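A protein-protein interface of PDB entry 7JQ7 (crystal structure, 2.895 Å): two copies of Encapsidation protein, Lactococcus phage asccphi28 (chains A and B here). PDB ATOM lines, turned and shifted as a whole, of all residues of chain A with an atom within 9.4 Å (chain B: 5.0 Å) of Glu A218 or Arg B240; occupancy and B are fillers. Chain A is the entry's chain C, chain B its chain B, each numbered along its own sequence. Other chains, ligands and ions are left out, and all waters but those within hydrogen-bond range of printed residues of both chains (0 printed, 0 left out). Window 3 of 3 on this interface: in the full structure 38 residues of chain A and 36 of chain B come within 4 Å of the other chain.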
ATOM      1  N   THR A  17      29.960  10.349 -12.618  1.00  0.00           N
ATOM      2  CA  THR A  17      28.787   9.528 -12.866  1.00  0.00           C
ATOM      3  C   THR A  17      29.207   8.149 -13.388  1.00  0.00           C
ATOM      4  O   THR A  17      30.348   7.926 -13.802  1.00  0.00           O
ATOM      5  CB  THR A  17      27.835  10.223 -13.840  1.00  0.00           C
ATOM      6  OG1 THR A  17      26.649   9.430 -13.991  1.00  0.00           O
ATOM      7  CG2 THR A  17      28.471  10.430 -15.201  1.00  0.00           C
ATOM      8  N   ASP A  18      28.262   7.215 -13.369  1.00  0.00           N
ATOM      9  CA  ASP A  18      28.521   5.829 -13.742  1.00  0.00           C
ATOM     10  C   ASP A  18      28.450   5.583 -15.247  1.00  0.00           C
ATOM     11  O   ASP A  18      28.720   4.460 -15.686  1.00  0.00           O
ATOM     12  CB  ASP A  18      27.537   4.898 -13.030  1.00  0.00           C
ATOM     13  CG  ASP A  18      27.762   4.850 -11.536  1.00  0.00           C
ATOM     14  OD1 ASP A  18      28.422   5.773 -11.007  1.00  0.00           O
ATOM     15  OD2 ASP A  18      27.287   3.889 -10.893  1.00  0.00           O
ATOM     16  N   ASP A  19      28.081   6.582 -16.039  1.00  0.00           N
ATOM     17  CA  ASP A  19      27.976   6.414 -17.479  1.00  0.00           C
ATOM     18  C   ASP A  19      29.356   6.412 -18.129  1.00  0.00           C
ATOM     19  O   ASP A  19      30.358   6.819 -17.533  1.00  0.00           O
ATOM     20  CB  ASP A  19      27.108   7.520 -18.078  1.00  0.00           C
ATOM     21  CG  ASP A  19      25.630   7.331 -17.770  1.00  0.00           C
ATOM     22  OD1 ASP A  19      25.089   6.247 -18.090  1.00  0.00           O
ATOM     23  OD2 ASP A  19      25.012   8.255 -17.195  1.00  0.00           O
ATOM     24  N   ARG A  20      29.401   5.901 -19.361  1.00  0.00           N
ATOM     25  CA  ARG A  20      30.654   5.766 -20.087  1.00  0.00           C
ATOM     26  C   ARG A  20      30.664   6.410 -21.465  1.00  0.00           C
ATOM     27  O   ARG A  20      31.725   6.426 -22.100  1.00  0.00           O
ATOM     28  CB  ARG A  20      31.017   4.284 -20.251  1.00  0.00           C
ATOM     29  CG  ARG A  20      31.247   3.575 -18.941  1.00  0.00           C
ATOM     30  CD  ARG A  20      31.767   2.172 -19.154  1.00  0.00           C
ATOM     31  NE  ARG A  20      32.135   1.548 -17.885  1.00  0.00           N
ATOM     32  CZ  ARG A  20      33.301   1.723 -17.269  1.00  0.00           C
ATOM     33  NH1 ARG A  20      34.227   2.507 -17.803  1.00  0.00           N
ATOM     34  NH2 ARG A  20      33.538   1.108 -16.117  1.00  0.00           N
ATOM     35  N   ILE A  21      29.544   6.944 -21.945  1.00  0.00           N
ATOM     36  CA  ILE A  21      29.477   7.608 -23.244  1.00  0.00           C
ATOM     37  C   ILE A  21      29.072   9.056 -23.015  1.00  0.00           C
ATOM     38  O   ILE A  21      27.989   9.325 -22.481  1.00  0.00           O
ATOM     39  CB  ILE A  21      28.500   6.910 -24.200  1.00  0.00           C
ATOM     40  CG1 ILE A  21      28.947   5.469 -24.431  1.00  0.00           C
ATOM     41  CG2 ILE A  21      28.415   7.673 -25.508  1.00  0.00           C
ATOM     42  CD1 ILE A  21      28.024   4.683 -25.330  1.00  0.00           C
ATOM     43  N   PHE A 165      27.437   6.617 -38.579  1.00  0.00           N
ATOM     44  CA  PHE A 165      27.313   6.084 -37.230  1.00  0.00           C
ATOM     45  C   PHE A 165      27.509   4.575 -37.199  1.00  0.00           C
ATOM     46  O   PHE A 165      27.972   4.034 -36.191  1.00  0.00           O
ATOM     47  CB  PHE A 165      25.962   6.447 -36.625  1.00  0.00           C
ATOM     48  CG  PHE A 165      25.936   6.337 -35.135  1.00  0.00           C
ATOM     49  CD1 PHE A 165      26.468   7.344 -34.346  1.00  0.00           C
ATOM     50  CD2 PHE A 165      25.392   5.225 -34.520  1.00  0.00           C
ATOM     51  CE1 PHE A 165      26.452   7.245 -32.971  1.00  0.00           C
ATOM     52  CE2 PHE A 165      25.371   5.118 -33.144  1.00  0.00           C
ATOM     53  CZ  PHE A 165      25.902   6.128 -32.367  1.00  0.00           C
ATOM     54  N   LEU A 169      30.397   2.698 -34.855  1.00  0.00           N
ATOM     55  CA  LEU A 169      30.163   1.557 -33.976  1.00  0.00           C
ATOM     56  C   LEU A 169      31.107   0.407 -34.304  1.00  0.00           C
ATOM     57  O   LEU A 169      31.662  -0.226 -33.398  1.00  0.00           O
ATOM     58  CB  LEU A 169      28.709   1.100 -34.069  1.00  0.00           C
ATOM     59  CG  LEU A 169      27.661   1.986 -33.400  1.00  0.00           C
ATOM     60  CD1 LEU A 169      26.286   1.444 -33.711  1.00  0.00           C
ATOM     61  CD2 LEU A 169      27.860   2.054 -31.899  1.00  0.00           C
ATOM     62  N   LYS A 176      37.503  -1.758 -28.886  1.00  0.00           N
ATOM     63  CA  LYS A 176      37.059  -2.272 -27.593  1.00  0.00           C
ATOM     64  C   LYS A 176      36.652  -3.727 -27.776  1.00  0.00           C
ATOM     65  O   LYS A 176      35.606  -4.015 -28.369  1.00  0.00           O
ATOM     66  CB  LYS A 176      35.895  -1.436 -27.062  1.00  0.00           C
ATOM     67  CG  LYS A 176      35.157  -2.033 -25.881  1.00  0.00           C
ATOM     68  CD  LYS A 176      33.807  -1.336 -25.708  1.00  0.00           C
ATOM     69  CE  LYS A 176      33.053  -1.863 -24.500  1.00  0.00           C
ATOM     70  NZ  LYS A 176      32.743  -3.318 -24.636  1.00  0.00           N
ATOM     71  N   GLU A 180      35.128  -4.032 -20.126  1.00  0.00           N
ATOM     72  CA  GLU A 180      34.199  -3.270 -19.298  1.00  0.00           C
ATOM     73  C   GLU A 180      34.649  -1.817 -19.189  1.00  0.00           C
ATOM     74  O   GLU A 180      33.839  -0.894 -19.322  1.00  0.00           O
ATOM     75  CB  GLU A 180      34.080  -3.903 -17.909  1.00  0.00           C
ATOM     76  CG  GLU A 180      33.516  -5.322 -17.901  1.00  0.00           C
ATOM     77  CD  GLU A 180      32.079  -5.397 -18.388  1.00  0.00           C
ATOM     78  OE1 GLU A 180      31.375  -4.363 -18.352  1.00  0.00           O
ATOM     79  OE2 GLU A 180      31.655  -6.495 -18.809  1.00  0.00           O
ATOM     80  N   GLY A 200      22.161   8.758 -34.524  1.00  0.00           N
ATOM     81  CA  GLY A 200      22.551   7.474 -33.965  1.00  0.00           C
ATOM     82  C   GLY A 200      22.301   7.376 -32.475  1.00  0.00           C
ATOM     83  O   GLY A 200      21.803   6.361 -31.984  1.00  0.00           O
ATOM     84  N   LEU A 201      22.654   8.422 -31.732  1.00  0.00           N
ATOM     85  CA  LEU A 201      22.373   8.432 -30.307  1.00  0.00           C
ATOM     86  C   LEU A 201      20.882   8.495 -30.016  1.00  0.00           C
ATOM     87  O   LEU A 201      20.473   8.223 -28.885  1.00  0.00           O
ATOM     88  CB  LEU A 201      23.071   9.609 -29.632  1.00  0.00           C
ATOM     89  CG  LEU A 201      24.597   9.609 -29.618  1.00  0.00           C
ATOM     90  CD1 LEU A 201      25.106  10.905 -28.988  1.00  0.00           C
ATOM     91  CD2 LEU A 201      25.136   8.401 -28.876  1.00  0.00           C
ATOM     92  N   VAL A 215      22.331  16.371 -19.441  1.00  0.00           N
ATOM     93  CA  VAL A 215      21.246  15.444 -19.746  1.00  0.00           C
ATOM     94  C   VAL A 215      21.765  14.037 -19.485  1.00  0.00           C
ATOM     95  O   VAL A 215      22.858  13.683 -19.939  1.00  0.00           O
ATOM     96  CB  VAL A 215      20.742  15.565 -21.197  1.00  0.00           C
ATOM     97  CG1 VAL A 215      19.713  14.470 -21.490  1.00  0.00           C
ATOM     98  CG2 VAL A 215      20.165  16.947 -21.457  1.00  0.00           C
ATOM     99  N   LYS A 216      20.999  13.243 -18.748  1.00  0.00           N
ATOM    100  CA  LYS A 216      21.348  11.855 -18.483  1.00  0.00           C
ATOM    101  C   LYS A 216      20.424  10.951 -19.287  1.00  0.00           C
ATOM    102  O   LYS A 216      19.199  11.093 -19.223  1.00  0.00           O
ATOM    103  CB  LYS A 216      21.247  11.531 -16.993  1.00  0.00           C
ATOM    104  CG  LYS A 216      22.034  12.484 -16.111  1.00  0.00           C
ATOM    105  CD  LYS A 216      22.423  11.852 -14.773  1.00  0.00           C
ATOM    106  CE  LYS A 216      23.099  12.871 -13.859  1.00  0.00           C
ATOM    107  NZ  LYS A 216      23.540  12.257 -12.582  1.00  0.00           N
ATOM    108  N   ARG A 217      21.014  10.037 -20.050  1.00  0.00           N
ATOM    109  CA  ARG A 217      20.270   9.035 -20.795  1.00  0.00           C
ATOM    110  C   ARG A 217      20.802   7.662 -20.412  1.00  0.00           C
ATOM    111  O   ARG A 217      21.847   7.539 -19.765  1.00  0.00           O
ATOM    112  CB  ARG A 217      20.375   9.275 -22.301  1.00  0.00           C
ATOM    113  CG  ARG A 217      19.766  10.593 -22.751  1.00  0.00           C
ATOM    114  CD  ARG A 217      18.263  10.625 -22.551  1.00  0.00           C
ATOM    115  NE  ARG A 217      17.703  11.922 -22.923  1.00  0.00           N
ATOM    116  CZ  ARG A 217      17.379  12.264 -24.165  1.00  0.00           C
ATOM    117  NH1 ARG A 217      17.567  11.402 -25.155  1.00  0.00           N
ATOM    118  NH2 ARG A 217      16.873  13.465 -24.421  1.00  0.00           N
ATOM    119  N   GLU A 218      20.078   6.616 -20.825  1.00  0.00           N
ATOM    120  CA  GLU A 218      20.435   5.273 -20.384  1.00  0.00           C
ATOM    121  C   GLU A 218      21.853   4.924 -20.808  1.00  0.00           C
ATOM    122  O   GLU A 218      22.634   4.387 -20.013  1.00  0.00           O
ATOM    123  CB  GLU A 218      19.453   4.240 -20.937  1.00  0.00           C
ATOM    124  CG  GLU A 218      19.687   2.831 -20.387  1.00  0.00           C
ATOM    125  CD  GLU A 218      18.968   1.743 -21.177  1.00  0.00           C
ATOM    126  OE1 GLU A 218      18.545   2.006 -22.325  1.00  0.00           O
ATOM    127  OE2 GLU A 218      18.834   0.617 -20.651  1.00  0.00           O
ATOM    128  N   ASP A 219      22.213   5.239 -22.050  1.00  0.00           N
ATOM    129  CA  ASP A 219      23.499   4.830 -22.593  1.00  0.00           C
ATOM    130  C   ASP A 219      24.533   5.945 -22.605  1.00  0.00           C
ATOM    131  O   ASP A 219      25.713   5.666 -22.852  1.00  0.00           O
ATOM    132  CB  ASP A 219      23.336   4.295 -24.021  1.00  0.00           C
ATOM    133  CG  ASP A 219      22.379   3.140 -24.097  1.00  0.00           C
ATOM    134  OD1 ASP A 219      22.221   2.436 -23.079  1.00  0.00           O
ATOM    135  OD2 ASP A 219      21.789   2.929 -25.175  1.00  0.00           O
ATOM    136  N   TYR A 220      24.135   7.189 -22.351  1.00  0.00           N
ATOM    137  CA  TYR A 220      25.093   8.279 -22.448  1.00  0.00           C
ATOM    138  C   TYR A 220      24.600   9.494 -21.673  1.00  0.00           C
ATOM    139  O   TYR A 220      23.439   9.573 -21.262  1.00  0.00           O
ATOM    140  CB  TYR A 220      25.356   8.648 -23.912  1.00  0.00           C
ATOM    141  CG  TYR A 220      24.119   9.101 -24.652  1.00  0.00           C
ATOM    142  CD1 TYR A 220      23.816  10.455 -24.774  1.00  0.00           C
ATOM    143  CD2 TYR A 220      23.255   8.181 -25.227  1.00  0.00           C
ATOM    144  CE1 TYR A 220      22.683  10.875 -25.450  1.00  0.00           C
ATOM    145  CE2 TYR A 220      22.121   8.591 -25.904  1.00  0.00           C
ATOM    146  CZ  TYR A 220      21.840   9.934 -26.010  1.00  0.00           C
ATOM    147  OH  TYR A 220      20.712  10.337 -26.685  1.00  0.00           O
ATOM    148  N   CYS A 221      25.526  10.438 -21.480  1.00  0.00           N
ATOM    149  CA  CYS A 221      25.260  11.742 -20.895  1.00  0.00           C
ATOM    150  C   CYS A 221      25.597  12.809 -21.925  1.00  0.00           C
ATOM    151  O   CYS A 221      26.476  12.617 -22.774  1.00  0.00           O
ATOM    152  CB  CYS A 221      26.089  11.980 -19.635  1.00  0.00           C
ATOM    153  SG  CYS A 221      25.558  11.036 -18.187  1.00  0.00           S
ATOM    154  N   VAL A 222      24.893  13.935 -21.850  1.00  0.00           N
ATOM    155  CA  VAL A 222      25.138  15.074 -22.728  1.00  0.00           C
ATOM    156  C   VAL A 222      25.382  16.308 -21.871  1.00  0.00           C
ATOM    157  O   VAL A 222      24.560  16.635 -21.007  1.00  0.00           O
ATOM    158  CB  VAL A 222      23.957  15.305 -23.692  1.00  0.00           C
ATOM    159  CG1 VAL A 222      24.278  16.431 -24.655  1.00  0.00           C
ATOM    160  CG2 VAL A 222      23.622  14.021 -24.441  1.00  0.00           C
ATOM    161  N   LYS A 360      17.492   8.160 -38.347  1.00  0.00           N
ATOM    162  CA  LYS A 360      18.215   6.898 -38.450  1.00  0.00           C
ATOM    163  C   LYS A 360      18.102   6.326 -39.856  1.00  0.00           C
ATOM    164  O   LYS A 360      19.097   5.898 -40.453  1.00  0.00           O
ATOM    165  CB  LYS A 360      17.682   5.885 -37.440  1.00  0.00           C
ATOM    166  CG  LYS A 360      18.132   6.086 -36.019  1.00  0.00           C
ATOM    167  CD  LYS A 360      17.711   4.882 -35.180  1.00  0.00           C
ATOM    168  CE  LYS A 360      18.204   5.013 -33.757  1.00  0.00           C
ATOM    169  NZ  LYS A 360      17.635   6.244 -33.130  1.00  0.00           N
ATOM    170  N   MET B 234      24.206  -6.996 -22.282  1.00  0.00           N
ATOM    171  CA  MET B 234      23.342  -5.820 -22.282  1.00  0.00           C
ATOM    172  C   MET B 234      23.602  -4.949 -21.051  1.00  0.00           C
ATOM    173  O   MET B 234      22.965  -3.908 -20.867  1.00  0.00           O
ATOM    174  CB  MET B 234      21.875  -6.248 -22.341  1.00  0.00           C
ATOM    175  CG  MET B 234      21.569  -7.250 -23.454  1.00  0.00           C
ATOM    176  SD  MET B 234      21.773  -6.518 -25.261  1.00  0.00           S
ATOM    177  CE  MET B 234      22.369  -8.118 -26.203  1.00  0.00           C
ATOM    178  N   THR B 235      24.547  -5.383 -20.212  1.00  0.00           N
ATOM    179  CA  THR B 235      25.022  -4.534 -19.126  1.00  0.00           C
ATOM    180  C   THR B 235      25.913  -3.412 -19.648  1.00  0.00           C
ATOM    181  O   THR B 235      26.012  -2.350 -19.020  1.00  0.00           O
ATOM    182  CB  THR B 235      25.825  -5.369 -18.118  1.00  0.00           C
ATOM    183  OG1 THR B 235      25.461  -6.752 -18.238  1.00  0.00           O
ATOM    184  CG2 THR B 235      25.596  -4.905 -16.687  1.00  0.00           C
ATOM    185  N   ASP B 236      26.560  -3.628 -20.794  1.00  0.00           N
ATOM    186  CA  ASP B 236      27.503  -2.659 -21.344  1.00  0.00           C
ATOM    187  C   ASP B 236      26.766  -1.590 -22.143  1.00  0.00           C
ATOM    188  O   ASP B 236      26.000  -1.925 -23.052  1.00  0.00           O
ATOM    189  CB  ASP B 236      28.527  -3.361 -22.225  1.00  0.00           C
ATOM    190  CG  ASP B 236      29.763  -2.532 -22.442  1.00  0.00           C
ATOM    191  OD1 ASP B 236      29.659  -1.289 -22.382  1.00  0.00           O
ATOM    192  OD2 ASP B 236      30.841  -3.122 -22.652  1.00  0.00           O
ATOM    193  N   PRO B 237      26.975  -0.305 -21.849  1.00  0.00           N
ATOM    194  CA  PRO B 237      26.251   0.725 -22.610  1.00  0.00           C
ATOM    195  C   PRO B 237      26.544   0.683 -24.095  1.00  0.00           C
ATOM    196  O   PRO B 237      25.643   0.922 -24.909  1.00  0.00           O
ATOM    197  CB  PRO B 237      26.739   2.036 -21.971  1.00  0.00           C
ATOM    198  CG  PRO B 237      27.144   1.642 -20.587  1.00  0.00           C
ATOM    199  CD  PRO B 237      27.793   0.291 -20.778  1.00  0.00           C
ATOM    200  N   PHE B 238      27.790   0.394 -24.474  1.00  0.00           N
ATOM    201  CA  PHE B 238      28.142   0.359 -25.888  1.00  0.00           C
ATOM    202  C   PHE B 238      27.353  -0.710 -26.638  1.00  0.00           C
ATOM    203  O   PHE B 238      26.932  -0.492 -27.780  1.00  0.00           O
ATOM    204  CB  PHE B 238      29.645   0.119 -26.048  1.00  0.00           C
ATOM    205  CG  PHE B 238      30.495   1.245 -25.546  1.00  0.00           C
ATOM    206  CD1 PHE B 238      30.884   1.301 -24.224  1.00  0.00           C
ATOM    207  CD2 PHE B 238      30.903   2.248 -26.401  1.00  0.00           C
ATOM    208  CE1 PHE B 238      31.666   2.339 -23.764  1.00  0.00           C
ATOM    209  CE2 PHE B 238      31.685   3.286 -25.948  1.00  0.00           C
ATOM    210  CZ  PHE B 238      32.066   3.331 -24.627  1.00  0.00           C
ATOM    211  N   VAL B 239      27.137  -1.869 -26.014  1.00  0.00           N
ATOM    212  CA  VAL B 239      26.393  -2.931 -26.685  1.00  0.00           C
ATOM    213  C   VAL B 239      24.957  -2.489 -26.935  1.00  0.00           C
ATOM    214  O   VAL B 239      24.386  -2.746 -28.002  1.00  0.00           O
ATOM    215  CB  VAL B 239      26.428  -4.232 -25.860  1.00  0.00           C
ATOM    216  CG1 VAL B 239      25.588  -5.307 -26.555  1.00  0.00           C
ATOM    217  CG2 VAL B 239      27.844  -4.692 -25.614  1.00  0.00           C
ATOM    218  N   ARG B 240      24.338  -1.856 -25.935  1.00  0.00           N
ATOM    219  CA  ARG B 240      22.972  -1.377 -26.098  1.00  0.00           C
ATOM    220  C   ARG B 240      22.907  -0.325 -27.196  1.00  0.00           C
ATOM    221  O   ARG B 240      21.988  -0.334 -28.021  1.00  0.00           O
ATOM    222  CB  ARG B 240      22.454  -0.803 -24.780  1.00  0.00           C
ATOM    223  CG  ARG B 240      22.515  -1.761 -23.585  1.00  0.00           C
ATOM    224  CD  ARG B 240      21.639  -1.256 -22.440  1.00  0.00           C
ATOM    225  NE  ARG B 240      21.968   0.119 -22.062  1.00  0.00           N
ATOM    226  CZ  ARG B 240      22.794   0.479 -21.082  1.00  0.00           C
ATOM    227  NH1 ARG B 240      23.408  -0.433 -20.336  1.00  0.00           N
ATOM    228  NH2 ARG B 240      23.011   1.767 -20.853  1.00  0.00           N
ATOM    229  N   LEU B 241      23.880   0.589 -27.223  1.00  0.00           N
ATOM    230  CA  LEU B 241      23.900   1.618 -28.258  1.00  0.00           C
ATOM    231  C   LEU B 241      23.885   0.979 -29.638  1.00  0.00           C
ATOM    232  O   LEU B 241      23.140   1.404 -30.527  1.00  0.00           O
ATOM    233  CB  LEU B 241      25.140   2.497 -28.104  1.00  0.00           C
ATOM    234  CG  LEU B 241      25.264   3.683 -29.065  1.00  0.00           C
ATOM    235  CD1 LEU B 241      24.260   4.759 -28.685  1.00  0.00           C
ATOM    236  CD2 LEU B 241      26.674   4.248 -29.116  1.00  0.00           C
ATOM    237  N   GLY B 242      24.712  -0.048 -29.832  1.00  0.00           N
ATOM    238  CA  GLY B 242      24.704  -0.769 -31.090  1.00  0.00           C
ATOM    239  C   GLY B 242      23.418  -1.543 -31.298  1.00  0.00           C
ATOM    240  O   GLY B 242      22.915  -1.641 -32.419  1.00  0.00           O
ATOM    241  N   ALA B 243      22.873  -2.113 -30.222  1.00  0.00           N
ATOM    242  CA  ALA B 243      21.635  -2.871 -30.339  1.00  0.00           C
ATOM    243  C   ALA B 243      20.488  -1.981 -30.789  1.00  0.00           C
ATOM    244  O   ALA B 243      19.574  -2.448 -31.478  1.00  0.00           O
ATOM    245  CB  ALA B 243      21.300  -3.531 -29.005  1.00  0.00           C
ATOM    246  N   LYS B 244      20.520  -0.700 -30.415  1.00  0.00           N
ATOM    247  CA  LYS B 244      19.472   0.240 -30.781  1.00  0.00           C
ATOM    248  C   LYS B 244      19.576   0.718 -32.223  1.00  0.00           C
ATOM    249  O   LYS B 244      18.653   1.387 -32.701  1.00  0.00           O
ATOM    250  CB  LYS B 244      19.490   1.448 -29.844  1.00  0.00           C
ATOM    251  CG  LYS B 244      18.996   1.148 -28.438  1.00  0.00           C
ATOM    252  CD  LYS B 244      19.267   2.317 -27.511  1.00  0.00           C
ATOM    253  CE  LYS B 244      18.785   2.039 -26.102  1.00  0.00           C
ATOM    254  NZ  LYS B 244      19.145   3.165 -25.196  1.00  0.00           N
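Pro B237 touches one residue of chain A. Val B239 touches none of the printed residues of chain A. Of the printed residues of chain A, Gly B242 touches Leu A169 (3.8 Å). Of the printed residues of chain B, Leu A169 touches Leu B241 and Gly B242. Of the printed residues of chain B, Lys A176 touches Asp B236 and Phe B238. Of the printed residues of chain A, Phe B238 touches Ile A21 and Lys A176. Of the printed residues of chain B, Ile A21 touches Phe B238 (3.8 Å). The nearest printed residue of chain B that does not touch Glu A218 is Pro B237 (5.1 Å). The nearest residue of chain A that does not touch Arg B240 is Asp A19 (5.7 Å).
The backbone carbonyl oxygen of Thr B235 sits at hydrogen-bond distance from the guanidinium group of Arg B240, at 3.5 Å. The side-chain carboxylate of Asp B236 lies close to the backbone NH of Phe B238 (3.3 Å). The backbone carbonyl oxygen (O) of Ile A21 is in hydrogen-bond range of the backbone NH (N) of Cys A221 (2.9 Å). The side-chain hydroxyl (OH) of Tyr A220 is in hydrogen-bond range of the backbone carbonyl oxygen (O) of Leu A201 (3.1 Å).
NZ of Lys A176 lies within salt-bridge range of OD2 of Asp B236 (2.8 Å). OE2 of Glu A218 lies within salt-bridge range of NE of Arg B240. NH2 of Arg B240 lies within salt-bridge range of OD1 of Asp A219. OE1 of Glu A218 is in salt-bridge range of NZ of Lys B244 (3.2 Å). The side-chain carboxylate (OD2) of Asp A219 is in salt-bridge range of the side-chain amino group (NZ) of Lys B244, at 2.7 Å.
No position is printed for both chains.
Of the 11 printed residues of chain B, 7 touch a printed residue of chain A. Printed residues of chain B that touch a printed residue of chain A: Asp B236, Pro B237, Phe B238, Arg B240, Leu B241, Gly B242 and Lys B244. Hydrophobic or aromatic side chains of chain B that line the printed part of chain A: Pro B237, Phe B238 and Leu B241. Of the 20 printed residues of chain A, 8 touch a printed residue of chain B. Printed residues of chain A that touch a printed residue of chain B: Ile A21, Phe A165, Leu A169, Lys A176, Leu A201, Glu A218, Asp A219 and Lys A360. Hydrophobic or aromatic side chains of chain A within 4 Å of the printed part of chain B: Ile A21, Phe A165, Leu A169 and Leu A201. Among the printed residues, Asp or Glu carboxylates within 4 Å of a Lys or Arg side-chain nitrogen of the other chain: Lys A176 with Asp B236, Glu A218 with Arg B240, Glu A218 with Lys B244, Asp A219 with Arg B240 and Asp A219 with Lys B244.
Among the printed residues, pairs that only touch across the chains: Leu A169 with Leu B241, Asp A219 with Leu B241, Leu A201 with Leu B241, Leu A169 with Gly B242, Ile A21 with Phe B238, Lys A360 with Lys B244, Phe A165 with Leu B241, Lys A176 with Phe B238 and Asp A219 with Pro B237.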
